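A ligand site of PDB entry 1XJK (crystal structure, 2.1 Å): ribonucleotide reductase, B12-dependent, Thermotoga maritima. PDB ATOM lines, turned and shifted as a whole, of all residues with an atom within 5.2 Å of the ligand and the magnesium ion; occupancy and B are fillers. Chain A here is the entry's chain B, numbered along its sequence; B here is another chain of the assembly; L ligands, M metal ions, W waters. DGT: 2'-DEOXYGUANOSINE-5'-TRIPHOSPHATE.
No residue comes within 4 Å of the magnesium ion.
The nearest printed residue that does not touch the magnesium ion is Ser 142 (4.02 Å).
The backbone carbonyl oxygen of Val 201 of chain B sits at hydrogen-bond distance from a nitrogen (N1) of the ligand (2.6 Å).
OD1 of Asp 141 sits at hydrogen-bond distance from O3' of the ligand.
The side-chain hydroxyl (OG) of Ser 185 sits at hydrogen-bond distance from a nitrogen (N2) of the ligand (2.7 Å).
O of Val 200 of chain B lies within hydrogen-bond range of N2 of the ligand (2.8 Å).
The side-chain amino group (NZ) of Lys 158 of chain B lies within salt-bridge range of an oxygen (O1B) of the ligand (2.9 Å).
An oxygen (O1G) of the ligand is in salt-bridge range of the guanidinium group (NH1) of Arg 171, 2.9 Å away.
N of Ile 143 is in hydrogen-bond range of O2A of the ligand, at 3.1 Å.
The backbone NH (N) of Ala 178 is in hydrogen-bond range of an oxygen (O1G) of the ligand (3.1 Å).
Residues that only touch the ligand: Val 177 (3.3 Å), Leu 128 of chain B (3.3 Å), Ser 142 (3.3 Å), His 127 of chain B (3.4 Å), Phe 190 (3.5 Å) and Ala 184 (3.8 Å).
Hydrophobic or aromatic side chains within 4 Å of the ligand: Ile 143, Val 177, Ala 178, Ala 184, Phe 190, His 127 of chain B, Leu 128 of chain B and Val 201 of chain B.
Within 4 Å of the ligand: Asp 141, Ser 142, Ile 143, Arg 171, Val 177, Ala 178, Ala 184, Ser 185, Phe 190, His 127 of chain B, Leu 128 of chain B, Lys 158 of chain B, Val 200 of chain B and Val 201 of chain B.
Water W2 lies within hydrogen-bond range of an oxygen (O2A) of the ligand, the backbone NH of Glu 144 and the backbone NH of Ile 143.
Water W4 lies within hydrogen-bond range of O of Arg 171 (2.8 Å) and O3' of the ligand (2.9 Å).
Water W3 lies within hydrogen-bond range of NE2 of His 127 of chain B (2.9 Å) and O3G of the ligand (3.1 Å).
The side-chain carboxylate (OD2) of Asp 141 is in salt-bridge range of the guanidinium group (NH2) of Arg 171, at 2.6 Å.
The backbone carbonyl oxygen (O) of Lys 158 of chain B sits close to a ring nitrogen (ND1) of His 181, at 3.3 Å.
The backbone carbonyl oxygen (O) of Phe 176 lies within hydrogen-bond range of the guanidinium group (NH1) of Arg 171 (3.3 Å).
The magnesium ion is bound by an oxygen (O1A) of the ligand (1.8 Å), water W1 (2.0 Å), an oxygen (O2B) of the ligand (2.1 Å), water W5 (2.3 Å) and an oxygen (O2G) of the ligand (2.5 Å).
The magnesium ion has five donor atoms within binding distance.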
ATOM      1  N   ASP A 141     -23.044  20.328  13.754  1.00  0.00           N
ATOM      2  CA  ASP A 141     -22.228  19.341  14.494  1.00  0.00           C
ATOM      3  C   ASP A 141     -21.376  20.016  15.591  1.00  0.00           C
ATOM      4  O   ASP A 141     -20.136  20.047  15.507  1.00  0.00           O
ATOM      5  CB  ASP A 141     -21.355  18.558  13.508  1.00  0.00           C
ATOM      6  CG  ASP A 141     -20.525  17.491  14.158  1.00  0.00           C
ATOM      7  OD1 ASP A 141     -21.013  16.705  14.987  1.00  0.00           O
ATOM      8  OD2 ASP A 141     -19.359  17.374  13.778  1.00  0.00           O
ATOM      9  N   SER A 142     -22.051  20.613  16.570  1.00  0.00           N
ATOM     10  CA  SER A 142     -21.390  21.238  17.711  1.00  0.00           C
ATOM     11  C   SER A 142     -22.372  21.299  18.804  1.00  0.00           C
ATOM     12  O   SER A 142     -23.562  21.468  18.540  1.00  0.00           O
ATOM     13  CB  SER A 142     -20.986  22.687  17.406  1.00  0.00           C
ATOM     14  OG  SER A 142     -22.142  23.503  17.316  1.00  0.00           O
ATOM     15  N   ILE A 143     -21.891  21.213  20.040  1.00  0.00           N
ATOM     16  CA  ILE A 143     -22.752  21.252  21.220  1.00  0.00           C
ATOM     17  C   ILE A 143     -23.603  22.520  21.219  1.00  0.00           C
ATOM     18  O   ILE A 143     -24.782  22.473  21.502  1.00  0.00           O
ATOM     19  CB  ILE A 143     -21.877  21.115  22.492  1.00  0.00           C
ATOM     20  CG1 ILE A 143     -21.467  19.661  22.662  1.00  0.00           C
ATOM     21  CG2 ILE A 143     -22.604  21.674  23.756  1.00  0.00           C
ATOM     22  CD1 ILE A 143     -22.636  18.780  22.879  1.00  0.00           C
ATOM     23  N   GLU A 144     -22.995  23.650  20.851  1.00  0.00           N
ATOM     24  CA  GLU A 144     -23.728  24.906  20.687  1.00  0.00           C
ATOM     25  C   GLU A 144     -24.988  24.767  19.767  1.00  0.00           C
ATOM     26  O   GLU A 144     -26.117  25.084  20.158  1.00  0.00           O
ATOM     27  CB  GLU A 144     -22.762  25.928  20.110  1.00  0.00           C
ATOM     28  CG  GLU A 144     -23.374  27.130  19.423  1.00  0.00           C
ATOM     29  CD  GLU A 144     -23.805  28.252  20.366  1.00  0.00           C
ATOM     30  OE1 GLU A 144     -23.189  28.346  21.446  1.00  0.00           O
ATOM     31  OE2 GLU A 144     -24.762  29.049  20.012  1.00  0.00           O
ATOM     32  N   ILE A 146     -26.315  21.918  18.596  1.00  0.00           N
ATOM     33  CA  ILE A 146     -27.277  20.916  19.043  1.00  0.00           C
ATOM     34  C   ILE A 146     -28.334  21.534  19.977  1.00  0.00           C
ATOM     35  O   ILE A 146     -29.523  21.220  19.876  1.00  0.00           O
ATOM     36  CB  ILE A 146     -26.594  19.754  19.732  1.00  0.00           C
ATOM     37  CG1 ILE A 146     -25.800  18.942  18.704  1.00  0.00           C
ATOM     38  CG2 ILE A 146     -27.624  18.812  20.417  1.00  0.00           C
ATOM     39  CD1 ILE A 146     -24.860  17.944  19.347  1.00  0.00           C
ATOM     40  N   LEU A 170     -24.180  15.437  12.753  1.00  0.00           N
ATOM     41  CA  LEU A 170     -23.533  14.999  13.978  1.00  0.00           C
ATOM     42  C   LEU A 170     -22.645  13.781  13.790  1.00  0.00           C
ATOM     43  O   LEU A 170     -23.131  12.668  13.555  1.00  0.00           O
ATOM     44  CB  LEU A 170     -24.575  14.703  15.056  1.00  0.00           C
ATOM     45  CG  LEU A 170     -25.659  15.757  15.261  1.00  0.00           C
ATOM     46  CD1 LEU A 170     -26.563  15.362  16.404  1.00  0.00           C
ATOM     47  CD2 LEU A 170     -25.040  17.127  15.464  1.00  0.00           C
ATOM     48  N   ARG A 171     -21.325  13.992  13.978  1.00  0.00           N
ATOM     49  CA  ARG A 171     -20.309  12.942  13.877  1.00  0.00           C
ATOM     50  C   ARG A 171     -20.713  11.726  14.679  1.00  0.00           C
ATOM     51  O   ARG A 171     -21.354  11.860  15.722  1.00  0.00           O
ATOM     52  CB  ARG A 171     -18.910  13.477  14.255  1.00  0.00           C
ATOM     53  CG  ARG A 171     -18.648  13.780  15.723  1.00  0.00           C
ATOM     54  CD  ARG A 171     -17.405  14.674  15.896  1.00  0.00           C
ATOM     55  NE  ARG A 171     -17.532  15.936  15.147  1.00  0.00           N
ATOM     56  CZ  ARG A 171     -16.785  17.031  15.350  1.00  0.00           C
ATOM     57  NH1 ARG A 171     -15.788  17.014  16.216  1.00  0.00           N
ATOM     58  NH2 ARG A 171     -17.006  18.126  14.656  1.00  0.00           N
ATOM     59  N   PHE A 176     -13.283  11.806  17.201  1.00  0.00           N
ATOM     60  CA  PHE A 176     -12.414  12.735  17.925  1.00  0.00           C
ATOM     61  C   PHE A 176     -13.148  14.061  18.091  1.00  0.00           C
ATOM     62  O   PHE A 176     -13.856  14.500  17.185  1.00  0.00           O
ATOM     63  CB  PHE A 176     -11.081  12.973  17.156  1.00  0.00           C
ATOM     64  CG  PHE A 176     -10.072  13.873  17.895  1.00  0.00           C
ATOM     65  CD1 PHE A 176      -9.809  15.178  17.429  1.00  0.00           C
ATOM     66  CD2 PHE A 176      -9.375  13.408  19.028  1.00  0.00           C
ATOM     67  CE1 PHE A 176      -8.875  16.024  18.118  1.00  0.00           C
ATOM     68  CE2 PHE A 176      -8.461  14.234  19.716  1.00  0.00           C
ATOM     69  CZ  PHE A 176      -8.194  15.535  19.264  1.00  0.00           C
ATOM     70  N   VAL A 177     -13.025  14.659  19.269  1.00  0.00           N
ATOM     71  CA  VAL A 177     -13.458  16.024  19.498  1.00  0.00           C
ATOM     72  C   VAL A 177     -12.233  16.758  19.970  1.00  0.00           C
ATOM     73  O   VAL A 177     -11.588  16.339  20.954  1.00  0.00           O
ATOM     74  CB  VAL A 177     -14.523  16.118  20.595  1.00  0.00           C
ATOM     75  CG1 VAL A 177     -14.976  17.555  20.720  1.00  0.00           C
ATOM     76  CG2 VAL A 177     -15.689  15.161  20.308  1.00  0.00           C
ATOM     77  N   ALA A 178     -11.870  17.823  19.267  1.00  0.00           N
ATOM     78  CA  ALA A 178     -10.738  18.630  19.702  1.00  0.00           C
ATOM     79  C   ALA A 178     -11.092  19.226  21.065  1.00  0.00           C
ATOM     80  O   ALA A 178     -11.850  20.211  21.131  1.00  0.00           O
ATOM     81  CB  ALA A 178     -10.429  19.698  18.685  1.00  0.00           C
ATOM     82  N   HIS A 181     -12.209  15.789  27.118  1.00  0.00           N
ATOM     83  CA  HIS A 181     -13.129  14.744  27.620  1.00  0.00           C
ATOM     84  C   HIS A 181     -13.361  13.582  26.632  1.00  0.00           C
ATOM     85  O   HIS A 181     -13.943  12.545  26.988  1.00  0.00           O
ATOM     86  CB  HIS A 181     -14.433  15.390  28.145  1.00  0.00           C
ATOM     87  CG  HIS A 181     -14.202  16.585  29.029  1.00  0.00           C
ATOM     88  ND1 HIS A 181     -13.690  17.775  28.548  1.00  0.00           N
ATOM     89  CD2 HIS A 181     -14.405  16.765  30.353  1.00  0.00           C
ATOM     90  CE1 HIS A 181     -13.587  18.636  29.541  1.00  0.00           C
ATOM     91  NE2 HIS A 181     -14.012  18.058  30.645  1.00  0.00           N
ATOM     92  N   LYS A 183     -14.582  11.989  23.246  1.00  0.00           N
ATOM     93  CA  LYS A 183     -15.293  11.404  22.133  1.00  0.00           C
ATOM     94  C   LYS A 183     -16.729  11.962  21.951  1.00  0.00           C
ATOM     95  O   LYS A 183     -17.408  12.315  22.923  1.00  0.00           O
ATOM     96  CB  LYS A 183     -15.300   9.864  22.314  1.00  0.00           C
ATOM     97  CG  LYS A 183     -13.965   9.175  21.883  1.00  0.00           C
ATOM     98  CD  LYS A 183     -13.630   7.944  22.728  1.00  0.00           C
ATOM     99  CE  LYS A 183     -12.645   7.013  22.016  1.00  0.00           C
ATOM    100  NZ  LYS A 183     -13.393   6.008  21.172  1.00  0.00           N
ATOM    101  N   ALA A 184     -17.156  12.075  20.680  1.00  0.00           N
ATOM    102  CA  ALA A 184     -18.571  12.390  20.322  1.00  0.00           C
ATOM    103  C   ALA A 184     -19.471  11.258  20.731  1.00  0.00           C
ATOM    104  O   ALA A 184     -19.109  10.110  20.593  1.00  0.00           O
ATOM    105  CB  ALA A 184     -18.666  12.628  18.868  1.00  0.00           C
ATOM    106  N   SER A 185     -20.650  11.531  21.264  1.00  0.00           N
ATOM    107  CA  SER A 185     -21.569  10.439  21.643  1.00  0.00           C
ATOM    108  C   SER A 185     -22.466  10.009  20.467  1.00  0.00           C
ATOM    109  O   SER A 185     -23.092   8.956  20.538  1.00  0.00           O
ATOM    110  CB  SER A 185     -22.417  10.821  22.860  1.00  0.00           C
ATOM    111  OG  SER A 185     -23.008  12.108  22.650  1.00  0.00           O
ATOM    112  N   PHE A 190     -27.905  12.277  21.185  1.00  0.00           N
ATOM    113  CA  PHE A 190     -28.533  13.603  21.165  1.00  0.00           C
ATOM    114  C   PHE A 190     -30.037  13.657  20.844  1.00  0.00           C
ATOM    115  O   PHE A 190     -30.755  14.467  21.438  1.00  0.00           O
ATOM    116  CB  PHE A 190     -27.770  14.547  20.248  1.00  0.00           C
ATOM    117  CG  PHE A 190     -26.431  14.879  20.767  1.00  0.00           C
ATOM    118  CD1 PHE A 190     -26.295  15.684  21.918  1.00  0.00           C
ATOM    119  CD2 PHE A 190     -25.286  14.312  20.206  1.00  0.00           C
ATOM    120  CE1 PHE A 190     -24.990  15.949  22.473  1.00  0.00           C
ATOM    121  CE2 PHE A 190     -23.987  14.554  20.764  1.00  0.00           C
ATOM    122  CZ  PHE A 190     -23.857  15.385  21.878  1.00  0.00           C
ATOM    123  N   HIS B 127     -11.168  28.413  22.442  1.00  0.00           N
ATOM    124  CA  HIS B 127     -12.485  28.462  23.055  1.00  0.00           C
ATOM    125  C   HIS B 127     -12.669  27.398  24.143  1.00  0.00           C
ATOM    126  O   HIS B 127     -13.672  27.393  24.852  1.00  0.00           O
ATOM    127  CB  HIS B 127     -13.550  28.275  21.961  1.00  0.00           C
ATOM    128  CG  HIS B 127     -13.432  26.978  21.221  1.00  0.00           C
ATOM    129  ND1 HIS B 127     -14.477  26.075  21.115  1.00  0.00           N
ATOM    130  CD2 HIS B 127     -12.387  26.414  20.564  1.00  0.00           C
ATOM    131  CE1 HIS B 127     -14.075  25.014  20.431  1.00  0.00           C
ATOM    132  NE2 HIS B 127     -12.815  25.191  20.081  1.00  0.00           N
ATOM    133  N   LEU B 128     -11.721  26.487  24.270  1.00  0.00           N
ATOM    134  CA  LEU B 128     -11.789  25.451  25.266  1.00  0.00           C
ATOM    135  C   LEU B 128     -10.841  25.731  26.453  1.00  0.00           C
ATOM    136  O   LEU B 128     -10.713  24.912  27.317  1.00  0.00           O
ATOM    137  CB  LEU B 128     -11.435  24.106  24.664  1.00  0.00           C
ATOM    138  CG  LEU B 128     -11.994  23.665  23.322  1.00  0.00           C
ATOM    139  CD1 LEU B 128     -11.227  22.413  22.944  1.00  0.00           C
ATOM    140  CD2 LEU B 128     -13.490  23.389  23.432  1.00  0.00           C
ATOM    141  N   LYS B 158     -19.385  20.731  28.977  1.00  0.00           N
ATOM    142  CA  LYS B 158     -18.443  20.249  27.983  1.00  0.00           C
ATOM    143  C   LYS B 158     -16.983  20.678  28.239  1.00  0.00           C
ATOM    144  O   LYS B 158     -16.039  19.954  27.959  1.00  0.00           O
ATOM    145  CB  LYS B 158     -18.870  20.782  26.622  1.00  0.00           C
ATOM    146  CG  LYS B 158     -17.899  20.434  25.505  1.00  0.00           C
ATOM    147  CD  LYS B 158     -17.887  21.497  24.492  1.00  0.00           C
ATOM    148  CE  LYS B 158     -16.916  21.149  23.375  1.00  0.00           C
ATOM    149  NZ  LYS B 158     -16.882  22.355  22.488  1.00  0.00           N
ATOM    150  N   VAL B 200     -26.192  13.012  28.592  1.00  0.00           N
ATOM    151  CA  VAL B 200     -25.657  12.831  27.292  1.00  0.00           C
ATOM    152  C   VAL B 200     -24.331  13.596  27.087  1.00  0.00           C
ATOM    153  O   VAL B 200     -23.422  13.024  26.502  1.00  0.00           O
ATOM    154  CB  VAL B 200     -26.697  13.128  26.155  1.00  0.00           C
ATOM    155  CG1 VAL B 200     -25.991  13.308  24.780  1.00  0.00           C
ATOM    156  CG2 VAL B 200     -27.789  12.061  26.101  1.00  0.00           C
ATOM    157  N   VAL B 201     -24.216  14.850  27.527  1.00  0.00           N
ATOM    158  CA  VAL B 201     -22.918  15.521  27.394  1.00  0.00           C
ATOM    159  C   VAL B 201     -21.802  14.775  28.113  1.00  0.00           C
ATOM    160  O   VAL B 201     -20.715  14.642  27.597  1.00  0.00           O
ATOM    161  CB  VAL B 201     -22.953  17.045  27.769  1.00  0.00           C
ATOM    162  CG1 VAL B 201     -21.568  17.637  27.739  1.00  0.00           C
ATOM    163  CG2 VAL B 201     -23.817  17.819  26.801  1.00  0.00           C
ATOM    164  N   LYS B 202     -22.096  14.224  29.285  1.00  0.00           N
ATOM    165  CA  LYS B 202     -21.129  13.484  30.052  1.00  0.00           C
ATOM    166  C   LYS B 202     -21.059  11.994  29.715  1.00  0.00           C
ATOM    167  O   LYS B 202     -20.410  11.222  30.433  1.00  0.00           O
ATOM    168  CB  LYS B 202     -21.429  13.696  31.510  1.00  0.00           C
ATOM    169  CG  LYS B 202     -21.353  15.170  31.879  1.00  0.00           C
ATOM    170  CD  LYS B 202     -20.889  15.374  33.294  1.00  0.00           C
ATOM    171  CE  LYS B 202     -19.423  15.773  33.370  1.00  0.00           C
ATOM    172  NZ  LYS B 202     -19.256  16.332  34.729  1.00  0.00           N
ATOM    173  N   GLN B 203     -21.706  11.583  28.631  1.00  0.00           N
ATOM    174  CA  GLN B 203     -21.765  10.182  28.240  1.00  0.00           C
ATOM    175  C   GLN B 203     -20.382   9.610  27.953  1.00  0.00           C
ATOM    176  O   GLN B 203     -19.774   9.927  26.909  1.00  0.00           O
ATOM    177  CB  GLN B 203     -22.642  10.013  27.005  1.00  0.00           C
ATOM    178  CG  GLN B 203     -23.101   8.593  26.808  1.00  0.00           C
ATOM    179  CD  GLN B 203     -23.925   8.451  25.568  1.00  0.00           C
ATOM    180  OE1 GLN B 203     -25.131   8.737  25.566  1.00  0.00           O
ATOM    181  NE2 GLN B 203     -23.271   8.017  24.485  1.00  0.00           N
HETATM  182  PG  DGT L   1     -14.307  20.127  17.098  1.00  0.00           P
HETATM  183  O1G DGT L   1     -13.643  18.841  16.889  1.00  0.00           O
HETATM  184  O2G DGT L   1     -15.670  20.375  16.578  1.00  0.00           O
HETATM  185  O3G DGT L   1     -13.487  21.412  16.543  1.00  0.00           O
HETATM  186  O3B DGT L   1     -14.275  20.285  18.693  1.00  0.00           O
HETATM  187  PB  DGT L   1     -15.243  21.376  19.456  1.00  0.00           P
HETATM  188  O1B DGT L   1     -14.663  21.727  20.778  1.00  0.00           O
HETATM  189  O2B DGT L   1     -15.593  22.477  18.500  1.00  0.00           O
HETATM  190  O3A DGT L   1     -16.571  20.312  19.781  1.00  0.00           O
HETATM  191  PA  DGT L   1     -18.092  20.685  19.290  1.00  0.00           P
HETATM  192  O1A DGT L   1     -17.951  21.449  18.070  1.00  0.00           O
HETATM  193  O2A DGT L   1     -18.856  21.228  20.379  1.00  0.00           O
HETATM  194  O5' DGT L   1     -18.613  19.226  19.170  1.00  0.00           O
HETATM  195  C5' DGT L   1     -18.424  18.509  17.993  1.00  0.00           C
HETATM  196  C4' DGT L   1     -19.255  17.201  18.031  1.00  0.00           C
HETATM  197  O4' DGT L   1     -18.776  16.434  19.167  1.00  0.00           O
HETATM  198  C3' DGT L   1     -20.758  17.328  18.196  1.00  0.00           C
HETATM  199  O3' DGT L   1     -21.400  16.151  17.630  1.00  0.00           O
HETATM  200  C2' DGT L   1     -20.879  17.262  19.710  1.00  0.00           C
HETATM  201  C1' DGT L   1     -19.786  16.239  20.135  1.00  0.00           C
HETATM  202  N9  DGT L   1     -19.234  16.577  21.520  1.00  0.00           N
HETATM  203  C8  DGT L   1     -18.345  17.569  21.801  1.00  0.00           C
HETATM  204  N7  DGT L   1     -18.168  17.601  23.147  1.00  0.00           N
HETATM  205  C5  DGT L   1     -18.929  16.606  23.664  1.00  0.00           C
HETATM  206  C6  DGT L   1     -19.177  16.176  24.967  1.00  0.00           C
HETATM  207  O6  DGT L   1     -18.621  16.620  25.975  1.00  0.00           O
HETATM  208  N1  DGT L   1     -20.058  15.161  25.170  1.00  0.00           N
HETATM  209  C2  DGT L   1     -20.736  14.549  24.155  1.00  0.00           C
HETATM  210  N2  DGT L   1     -21.584  13.548  24.495  1.00  0.00           N
HETATM  211  N3  DGT L   1     -20.489  14.990  22.922  1.00  0.00           N
HETATM  212  C4  DGT L   1     -19.610  15.988  22.656  1.00  0.00           C
HETATM  213 MG    MG M   1     -17.007  22.470  16.902  1.00  0.00          MG
HETATM  214  O   HOH W   1     -15.456  22.566  15.723  1.00  0.00           O
HETATM  215  O   HOH W   2     -19.835  23.853  20.777  1.00  0.00           O
HETATM  216  O   HOH W   3     -11.871  23.785  17.720  1.00  0.00           O
HETATM  217  O   HOH W   4     -21.692  13.326  18.025  1.00  0.00           O
HETATM  218  O   HOH W   5     -17.929  21.730  14.985  1.00  0.00           O
